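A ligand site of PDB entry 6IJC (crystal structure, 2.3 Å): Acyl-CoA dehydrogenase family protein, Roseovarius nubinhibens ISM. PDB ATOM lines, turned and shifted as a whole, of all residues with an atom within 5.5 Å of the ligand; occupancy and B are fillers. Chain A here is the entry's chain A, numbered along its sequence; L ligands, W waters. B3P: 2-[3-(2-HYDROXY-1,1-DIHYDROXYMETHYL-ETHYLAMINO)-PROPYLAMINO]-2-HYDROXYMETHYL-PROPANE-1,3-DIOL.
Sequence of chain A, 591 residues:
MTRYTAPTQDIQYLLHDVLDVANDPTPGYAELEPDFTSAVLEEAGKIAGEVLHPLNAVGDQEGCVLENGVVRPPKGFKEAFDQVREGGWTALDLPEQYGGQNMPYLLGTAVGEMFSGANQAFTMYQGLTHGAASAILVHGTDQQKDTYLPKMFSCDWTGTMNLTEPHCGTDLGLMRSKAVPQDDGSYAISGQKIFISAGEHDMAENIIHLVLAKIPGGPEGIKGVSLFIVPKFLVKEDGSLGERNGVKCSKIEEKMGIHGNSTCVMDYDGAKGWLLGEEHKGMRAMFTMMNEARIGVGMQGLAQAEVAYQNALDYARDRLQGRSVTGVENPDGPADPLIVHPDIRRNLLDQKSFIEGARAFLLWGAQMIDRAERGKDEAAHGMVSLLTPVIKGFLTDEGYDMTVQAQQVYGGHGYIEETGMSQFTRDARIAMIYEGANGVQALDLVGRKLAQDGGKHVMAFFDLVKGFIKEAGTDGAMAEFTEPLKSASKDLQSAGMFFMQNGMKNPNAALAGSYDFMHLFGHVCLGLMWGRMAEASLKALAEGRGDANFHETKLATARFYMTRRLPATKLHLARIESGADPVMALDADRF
Tyr 105 touches the ligand (CE1 to O3, 3.2 Å).
CA of Gly 112 touches O1 of the ligand, 3.4 Å away.
Leu 128 touches the ligand.
O of Glu 292 touches O5 of the ligand, 3.8 Å away.
Gly 296 touches the ligand.
N of Val 297 touches O5 of the ligand (3.8 Å).
Hydrophobic or aromatic side chains within 4 Å of the ligand: Tyr 105, Leu 128, His 130, Ala 293 and Val 297.
11 residues have an atom within 4 Å of the ligand: Asp 93, Tyr 105, Gly 108, Gly 112, Gly 127, Leu 128, His 130, Glu 292, Ala 293, Gly 296 and Val 297.
The nearest printed residue that does not touch the ligand is Glu 435 (4.1 Å).
The side-chain carboxylate of Asp 93 lies within hydrogen-bond range of a ring nitrogen (NE2) of His 130, 2.6 Å away.
O of Tyr 105 is in hydrogen-bond range of OG1 of Thr 109.
OD2 of Asp 93 is in hydrogen-bond range of O3 of the ligand.
A ring nitrogen (NE2) of His 130 lies close to an oxygen (O3) of the ligand (3.2 Å).
The backbone carbonyl oxygen (O) of Gly 127 lies within hydrogen-bond range of a nitrogen (N1) of the ligand (3.1 Å).
O of Ala 293 is in hydrogen-bond range of O5 of the ligand (2.6 Å).
O of Gly 108 lies close to O2 of the ligand.
Water W4 lies within hydrogen-bond range of O2 of the ligand (2.9 Å) and O of Gly 108 (3.3 Å).
Water W2 lies within hydrogen-bond range of O2 of the ligand (3.1 Å), N of Leu 92 (3.2 Å) and OD1 of Asp 93 (3.3 Å).
Water W1 bridges OH of Tyr 105 (2.7 Å) and O of Glu 292 (3.0 Å).
Water W5 lies within hydrogen-bond range of the side-chain hydroxyl (OG1) of Thr 109 (2.7 Å) and the side-chain hydroxyl (OH) of Tyr 105 (3.1 Å).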
ATOM      1  N   LEU A  92      -8.610  14.407 -21.353  1.00  0.00           N
ATOM      2  CA  LEU A  92      -9.904  14.896 -20.867  1.00  0.00           C
ATOM      3  C   LEU A  92      -9.947  16.425 -20.796  1.00  0.00           C
ATOM      4  O   LEU A  92     -10.882  17.048 -21.302  1.00  0.00           O
ATOM      5  CB  LEU A  92     -10.153  14.293 -19.495  1.00  0.00           C
ATOM      6  CG  LEU A  92     -11.582  13.973 -19.156  1.00  0.00           C
ATOM      7  CD1 LEU A  92     -12.080  12.954 -20.135  1.00  0.00           C
ATOM      8  CD2 LEU A  92     -11.665  13.472 -17.735  1.00  0.00           C
ATOM      9  N   ASP A  93      -8.934  17.043 -20.181  1.00  0.00           N
ATOM     10  CA  ASP A  93      -8.918  18.475 -19.935  1.00  0.00           C
ATOM     11  C   ASP A  93      -7.970  19.228 -20.864  1.00  0.00           C
ATOM     12  O   ASP A  93      -7.621  20.378 -20.577  1.00  0.00           O
ATOM     13  CB  ASP A  93      -8.572  18.763 -18.466  1.00  0.00           C
ATOM     14  CG  ASP A  93      -7.254  18.113 -18.008  1.00  0.00           C
ATOM     15  OD1 ASP A  93      -6.484  17.598 -18.844  1.00  0.00           O
ATOM     16  OD2 ASP A  93      -6.990  18.123 -16.784  1.00  0.00           O
ATOM     17  N   TYR A 105     -10.314  21.467 -15.767  1.00  0.00           N
ATOM     18  CA  TYR A 105      -9.242  20.888 -14.953  1.00  0.00           C
ATOM     19  C   TYR A 105      -9.789  20.314 -13.657  1.00  0.00           C
ATOM     20  O   TYR A 105      -9.248  19.319 -13.144  1.00  0.00           O
ATOM     21  CB  TYR A 105      -8.169  21.943 -14.650  1.00  0.00           C
ATOM     22  CG  TYR A 105      -7.016  21.483 -13.774  1.00  0.00           C
ATOM     23  CD1 TYR A 105      -6.009  20.688 -14.276  1.00  0.00           C
ATOM     24  CD2 TYR A 105      -6.920  21.886 -12.440  1.00  0.00           C
ATOM     25  CE1 TYR A 105      -4.936  20.276 -13.493  1.00  0.00           C
ATOM     26  CE2 TYR A 105      -5.840  21.487 -11.653  1.00  0.00           C
ATOM     27  CZ  TYR A 105      -4.849  20.685 -12.187  1.00  0.00           C
ATOM     28  OH  TYR A 105      -3.790  20.261 -11.419  1.00  0.00           O
ATOM     29  N   GLY A 108     -10.855  16.788 -14.563  1.00  0.00           N
ATOM     30  CA  GLY A 108      -9.707  15.932 -14.784  1.00  0.00           C
ATOM     31  C   GLY A 108      -8.990  15.570 -13.496  1.00  0.00           C
ATOM     32  O   GLY A 108      -8.546  14.443 -13.315  1.00  0.00           O
ATOM     33  N   THR A 109      -8.876  16.543 -12.576  1.00  0.00           N
ATOM     34  CA  THR A 109      -8.306  16.287 -11.260  1.00  0.00           C
ATOM     35  C   THR A 109      -9.170  15.322 -10.466  1.00  0.00           C
ATOM     36  O   THR A 109      -8.655  14.392  -9.828  1.00  0.00           O
ATOM     37  CB  THR A 109      -8.117  17.615 -10.498  1.00  0.00           C
ATOM     38  OG1 THR A 109      -7.121  18.412 -11.156  1.00  0.00           O
ATOM     39  CG2 THR A 109      -7.711  17.387  -9.042  1.00  0.00           C
ATOM     40  N   VAL A 111     -11.183  13.016 -11.680  1.00  0.00           N
ATOM     41  CA  VAL A 111     -10.917  11.707 -12.293  1.00  0.00           C
ATOM     42  C   VAL A 111      -9.534  11.207 -11.890  1.00  0.00           C
ATOM     43  O   VAL A 111      -9.342  10.021 -11.592  1.00  0.00           O
ATOM     44  CB  VAL A 111     -11.071  11.802 -13.821  1.00  0.00           C
ATOM     45  CG1 VAL A 111     -10.701  10.495 -14.485  1.00  0.00           C
ATOM     46  CG2 VAL A 111     -12.481  12.208 -14.195  1.00  0.00           C
ATOM     47  N   GLY A 112      -8.532  12.102 -11.875  1.00  0.00           N
ATOM     48  CA  GLY A 112      -7.164  11.696 -11.608  1.00  0.00           C
ATOM     49  C   GLY A 112      -6.945  11.110 -10.232  1.00  0.00           C
ATOM     50  O   GLY A 112      -6.112  10.215 -10.059  1.00  0.00           O
ATOM     51  N   GLU A 113      -7.683  11.600  -9.222  1.00  0.00           N
ATOM     52  CA  GLU A 113      -7.532  11.012  -7.903  1.00  0.00           C
ATOM     53  C   GLU A 113      -7.957   9.550  -7.904  1.00  0.00           C
ATOM     54  O   GLU A 113      -7.373   8.734  -7.187  1.00  0.00           O
ATOM     55  CB  GLU A 113      -8.327  11.793  -6.837  1.00  0.00           C
ATOM     56  CG  GLU A 113      -7.987  11.375  -5.383  1.00  0.00           C
ATOM     57  CD  GLU A 113      -9.228  11.316  -4.487  1.00  0.00           C
ATOM     58  OE1 GLU A 113     -10.087  12.197  -4.626  1.00  0.00           O
ATOM     59  OE2 GLU A 113      -9.362  10.378  -3.675  1.00  0.00           O
ATOM     60  N   THR A 123      -0.703   5.228 -13.076  1.00  0.00           N
ATOM     61  CA  THR A 123      -1.221   6.540 -13.466  1.00  0.00           C
ATOM     62  C   THR A 123      -0.118   7.551 -13.775  1.00  0.00           C
ATOM     63  O   THR A 123      -0.351   8.495 -14.548  1.00  0.00           O
ATOM     64  CB  THR A 123      -2.147   7.063 -12.367  1.00  0.00           C
ATOM     65  OG1 THR A 123      -3.163   6.087 -12.108  1.00  0.00           O
ATOM     66  CG2 THR A 123      -2.786   8.379 -12.771  1.00  0.00           C
ATOM     67  N   MET A 124       1.083   7.372 -13.225  1.00  0.00           N
ATOM     68  CA  MET A 124       2.179   8.290 -13.518  1.00  0.00           C
ATOM     69  C   MET A 124       2.620   8.253 -14.977  1.00  0.00           C
ATOM     70  O   MET A 124       3.219   9.225 -15.444  1.00  0.00           O
ATOM     71  CB  MET A 124       3.387   7.995 -12.622  1.00  0.00           C
ATOM     72  CG  MET A 124       3.109   8.274 -11.149  1.00  0.00           C
ATOM     73  SD  MET A 124       4.473   7.789 -10.090  1.00  0.00           S
ATOM     74  CE  MET A 124       5.798   8.825 -10.698  1.00  0.00           C
ATOM     75  N   GLY A 127       0.240  10.667 -16.391  1.00  0.00           N
ATOM     76  CA  GLY A 127       0.394  11.935 -15.674  1.00  0.00           C
ATOM     77  C   GLY A 127       1.660  12.675 -16.042  1.00  0.00           C
ATOM     78  O   GLY A 127       1.653  13.909 -16.157  1.00  0.00           O
ATOM     79  N   LEU A 128       2.774  11.954 -16.210  1.00  0.00           N
ATOM     80  CA  LEU A 128       4.005  12.629 -16.630  1.00  0.00           C
ATOM     81  C   LEU A 128       3.888  13.129 -18.071  1.00  0.00           C
ATOM     82  O   LEU A 128       4.367  14.230 -18.394  1.00  0.00           O
ATOM     83  CB  LEU A 128       5.202  11.699 -16.475  1.00  0.00           C
ATOM     84  CG  LEU A 128       5.531  11.333 -15.032  1.00  0.00           C
ATOM     85  CD1 LEU A 128       6.235   9.999 -14.993  1.00  0.00           C
ATOM     86  CD2 LEU A 128       6.404  12.388 -14.386  1.00  0.00           C
ATOM     87  N   HIS A 130       1.037  14.038 -19.456  1.00  0.00           N
ATOM     88  CA  HIS A 130       0.208  15.240 -19.342  1.00  0.00           C
ATOM     89  C   HIS A 130       1.055  16.448 -18.970  1.00  0.00           C
ATOM     90  O   HIS A 130       0.849  17.544 -19.485  1.00  0.00           O
ATOM     91  CB  HIS A 130      -0.901  15.012 -18.309  1.00  0.00           C
ATOM     92  CG  HIS A 130      -2.040  15.991 -18.401  1.00  0.00           C
ATOM     93  ND1 HIS A 130      -1.905  17.323 -18.053  1.00  0.00           N
ATOM     94  CD2 HIS A 130      -3.323  15.826 -18.788  1.00  0.00           C
ATOM     95  CE1 HIS A 130      -3.062  17.932 -18.244  1.00  0.00           C
ATOM     96  NE2 HIS A 130      -3.934  17.053 -18.683  1.00  0.00           N
ATOM     97  N   GLY A 131       2.043  16.255 -18.092  1.00  0.00           N
ATOM     98  CA  GLY A 131       2.891  17.359 -17.684  1.00  0.00           C
ATOM     99  C   GLY A 131       3.858  17.769 -18.780  1.00  0.00           C
ATOM    100  O   GLY A 131       4.103  18.958 -19.001  1.00  0.00           O
ATOM    101  N   ALA A 132       4.410  16.787 -19.487  1.00  0.00           N
ATOM    102  CA  ALA A 132       5.333  17.103 -20.577  1.00  0.00           C
ATOM    103  C   ALA A 132       4.584  17.727 -21.765  1.00  0.00           C
ATOM    104  O   ALA A 132       5.112  18.646 -22.413  1.00  0.00           O
ATOM    105  CB  ALA A 132       6.091  15.839 -20.998  1.00  0.00           C
ATOM    106  N   MET A 161      10.037  14.506 -17.768  1.00  0.00           N
ATOM    107  CA  MET A 161      10.957  15.599 -17.475  1.00  0.00           C
ATOM    108  C   MET A 161      12.315  15.039 -17.079  1.00  0.00           C
ATOM    109  O   MET A 161      12.386  14.046 -16.342  1.00  0.00           O
ATOM    110  CB  MET A 161      10.416  16.469 -16.341  1.00  0.00           C
ATOM    111  CG  MET A 161       8.935  16.784 -16.447  1.00  0.00           C
ATOM    112  SD  MET A 161       8.591  17.900 -17.820  1.00  0.00           S
ATOM    113  CE  MET A 161       9.931  19.108 -17.637  1.00  0.00           C
ATOM    114  N   GLU A 292       0.041  23.343 -11.284  1.00  0.00           N
ATOM    115  CA  GLU A 292      -0.630  22.081 -11.611  1.00  0.00           C
ATOM    116  C   GLU A 292       0.228  20.872 -11.235  1.00  0.00           C
ATOM    117  O   GLU A 292      -0.307  19.847 -10.818  1.00  0.00           O
ATOM    118  CB  GLU A 292      -1.016  22.080 -13.093  1.00  0.00           C
ATOM    119  CG  GLU A 292      -2.140  23.074 -13.390  1.00  0.00           C
ATOM    120  CD  GLU A 292      -2.615  23.038 -14.847  1.00  0.00           C
ATOM    121  OE1 GLU A 292      -2.576  21.959 -15.467  1.00  0.00           O
ATOM    122  OE2 GLU A 292      -3.012  24.111 -15.379  1.00  0.00           O
ATOM    123  N   ALA A 293       1.555  20.974 -11.375  1.00  0.00           N
ATOM    124  CA  ALA A 293       2.398  19.883 -10.899  1.00  0.00           C
ATOM    125  C   ALA A 293       2.190  19.650  -9.393  1.00  0.00           C
ATOM    126  O   ALA A 293       1.997  18.513  -8.953  1.00  0.00           O
ATOM    127  CB  ALA A 293       3.872  20.171 -11.217  1.00  0.00           C
ATOM    128  N   ARG A 294       2.204  20.724  -8.613  1.00  0.00           N
ATOM    129  CA  ARG A 294       2.006  20.615  -7.166  1.00  0.00           C
ATOM    130  C   ARG A 294       0.660  19.975  -6.841  1.00  0.00           C
ATOM    131  O   ARG A 294       0.584  19.075  -5.983  1.00  0.00           O
ATOM    132  CB  ARG A 294       2.093  21.990  -6.508  1.00  0.00           C
ATOM    133  CG  ARG A 294       3.485  22.554  -6.371  1.00  0.00           C
ATOM    134  CD  ARG A 294       3.390  23.870  -5.609  1.00  0.00           C
ATOM    135  NE  ARG A 294       4.686  24.515  -5.453  1.00  0.00           N
ATOM    136  CZ  ARG A 294       5.000  25.695  -5.973  1.00  0.00           C
ATOM    137  NH1 ARG A 294       4.091  26.370  -6.685  1.00  0.00           N
ATOM    138  NH2 ARG A 294       6.201  26.205  -5.760  1.00  0.00           N
ATOM    139  N   ILE A 295      -0.415  20.430  -7.497  1.00  0.00           N
ATOM    140  CA  ILE A 295      -1.758  19.897  -7.244  1.00  0.00           C
ATOM    141  C   ILE A 295      -1.844  18.429  -7.622  1.00  0.00           C
ATOM    142  O   ILE A 295      -2.461  17.625  -6.918  1.00  0.00           O
ATOM    143  CB  ILE A 295      -2.820  20.713  -8.002  1.00  0.00           C
ATOM    144  CG1 ILE A 295      -3.030  22.076  -7.343  1.00  0.00           C
ATOM    145  CG2 ILE A 295      -4.131  19.916  -8.103  1.00  0.00           C
ATOM    146  CD1 ILE A 295      -4.113  22.965  -8.028  1.00  0.00           C
ATOM    147  N   GLY A 296      -1.226  18.049  -8.741  1.00  0.00           N
ATOM    148  CA  GLY A 296      -1.203  16.640  -9.124  1.00  0.00           C
ATOM    149  C   GLY A 296      -0.477  15.741  -8.134  1.00  0.00           C
ATOM    150  O   GLY A 296      -0.854  14.574  -7.962  1.00  0.00           O
ATOM    151  N   VAL A 297       0.561  16.244  -7.465  1.00  0.00           N
ATOM    152  CA  VAL A 297       1.288  15.397  -6.512  1.00  0.00           C
ATOM    153  C   VAL A 297       0.582  15.374  -5.165  1.00  0.00           C
ATOM    154  O   VAL A 297       0.546  14.334  -4.491  1.00  0.00           O
ATOM    155  CB  VAL A 297       2.757  15.850  -6.398  1.00  0.00           C
ATOM    156  CG1 VAL A 297       3.446  15.193  -5.185  1.00  0.00           C
ATOM    157  CG2 VAL A 297       3.498  15.510  -7.667  1.00  0.00           C
ATOM    158  N   MET A 299      -2.580  15.492  -4.988  1.00  0.00           N
ATOM    159  CA  MET A 299      -3.605  14.522  -5.350  1.00  0.00           C
ATOM    160  C   MET A 299      -3.111  13.090  -5.120  1.00  0.00           C
ATOM    161  O   MET A 299      -3.866  12.241  -4.637  1.00  0.00           O
ATOM    162  CB  MET A 299      -4.005  14.762  -6.803  1.00  0.00           C
ATOM    163  CG  MET A 299      -5.064  13.827  -7.346  1.00  0.00           C
ATOM    164  SD  MET A 299      -4.802  13.623  -9.124  1.00  0.00           S
ATOM    165  CE  MET A 299      -3.475  12.403  -9.100  1.00  0.00           C
ATOM    166  N   GLN A 300      -1.850  12.821  -5.454  1.00  0.00           N
ATOM    167  CA  GLN A 300      -1.306  11.486  -5.241  1.00  0.00           C
ATOM    168  C   GLN A 300      -1.280  11.118  -3.768  1.00  0.00           C
ATOM    169  O   GLN A 300      -1.591   9.975  -3.394  1.00  0.00           O
ATOM    170  CB  GLN A 300       0.100  11.370  -5.827  1.00  0.00           C
ATOM    171  CG  GLN A 300       0.156  11.310  -7.337  1.00  0.00           C
ATOM    172  CD  GLN A 300       1.579  11.130  -7.830  1.00  0.00           C
ATOM    173  OE1 GLN A 300       2.481  11.849  -7.416  1.00  0.00           O
ATOM    174  NE2 GLN A 300       1.779  10.164  -8.712  1.00  0.00           N
ATOM    175  N   TYR A 434       9.547  14.069  -4.398  1.00  0.00           N
ATOM    176  CA  TYR A 434       9.710  14.631  -5.704  1.00  0.00           C
ATOM    177  C   TYR A 434       8.815  15.802  -6.028  1.00  0.00           C
ATOM    178  O   TYR A 434       7.958  16.145  -5.268  1.00  0.00           O
ATOM    179  CB  TYR A 434       9.717  13.535  -6.760  1.00  0.00           C
ATOM    180  CG  TYR A 434       8.406  13.069  -7.207  1.00  0.00           C
ATOM    181  CD1 TYR A 434       7.278  13.292  -6.493  1.00  0.00           C
ATOM    182  CD2 TYR A 434       8.294  12.401  -8.373  1.00  0.00           C
ATOM    183  CE1 TYR A 434       6.073  12.861  -6.918  1.00  0.00           C
ATOM    184  CE2 TYR A 434       7.094  11.977  -8.826  1.00  0.00           C
ATOM    185  CZ  TYR A 434       5.988  12.212  -8.085  1.00  0.00           C
ATOM    186  OH  TYR A 434       4.807  11.795  -8.568  1.00  0.00           O
ATOM    187  N   GLU A 435       9.062  16.418  -7.179  1.00  0.00           N
ATOM    188  CA  GLU A 435       8.318  17.544  -7.645  1.00  0.00           C
ATOM    189  C   GLU A 435       8.430  18.636  -6.624  1.00  0.00           C
ATOM    190  O   GLU A 435       7.499  19.332  -6.381  1.00  0.00           O
ATOM    191  CB  GLU A 435       6.884  17.141  -7.842  1.00  0.00           C
ATOM    192  CG  GLU A 435       6.091  18.154  -8.629  1.00  0.00           C
ATOM    193  CD  GLU A 435       6.669  18.384 -10.007  1.00  0.00           C
ATOM    194  OE1 GLU A 435       6.644  17.455 -10.825  1.00  0.00           O
ATOM    195  OE2 GLU A 435       7.159  19.489 -10.261  1.00  0.00           O
HETATM  196  C1  B3P L   1      -0.791  15.650 -14.109  1.00  0.00           C
HETATM  197  C2  B3P L   1      -2.249  15.398 -13.828  1.00  0.00           C
HETATM  198  C3  B3P L   1       0.251  15.307 -13.069  1.00  0.00           C
HETATM  199  N1  B3P L   1       1.650  15.361 -13.468  1.00  0.00           N
HETATM  200  C4  B3P L   1       2.598  14.898 -12.465  1.00  0.00           C
HETATM  201  C5  B3P L   1       3.903  14.615 -13.141  1.00  0.00           C
HETATM  202  C6  B3P L   1       2.926  15.940 -11.450  1.00  0.00           C
HETATM  203  C7  B3P L   1       2.104  13.634 -11.849  1.00  0.00           C
HETATM  204  N2  B3P L   1      -3.116  15.217 -14.998  1.00  0.00           N
HETATM  205  C8  B3P L   1      -4.506  15.548 -14.741  1.00  0.00           C
HETATM  206  C9  B3P L   1      -4.991  14.863 -13.491  1.00  0.00           C
HETATM  207  C10 B3P L   1      -5.291  15.065 -15.924  1.00  0.00           C
HETATM  208  C11 B3P L   1      -4.694  17.020 -14.556  1.00  0.00           C
HETATM  209  O1  B3P L   1      -4.840  13.487 -13.366  1.00  0.00           O
HETATM  210  O2  B3P L   1      -6.656  15.341 -16.029  1.00  0.00           O
HETATM  211  O3  B3P L   1      -4.451  17.894 -15.616  1.00  0.00           O
HETATM  212  O4  B3P L   1       4.186  15.343 -14.284  1.00  0.00           O
HETATM  213  O5  B3P L   1       1.934  16.754 -10.923  1.00  0.00           O
HETATM  214  O6  B3P L   1       1.883  12.590 -12.731  1.00  0.00           O
HETATM  215  O   HOH W   1      -2.288  18.244 -12.416  1.00  0.00           O
HETATM  216  O   HOH W   2      -6.414  14.330 -18.988  1.00  0.00           O
HETATM  217  O   HOH W   3      -2.775  12.762 -15.931  1.00  0.00           O
HETATM  218  O   HOH W   4      -7.214  12.521 -15.634  1.00  0.00           O
HETATM  219  O   HOH W   5      -4.627  17.269 -11.022  1.00  0.00           O
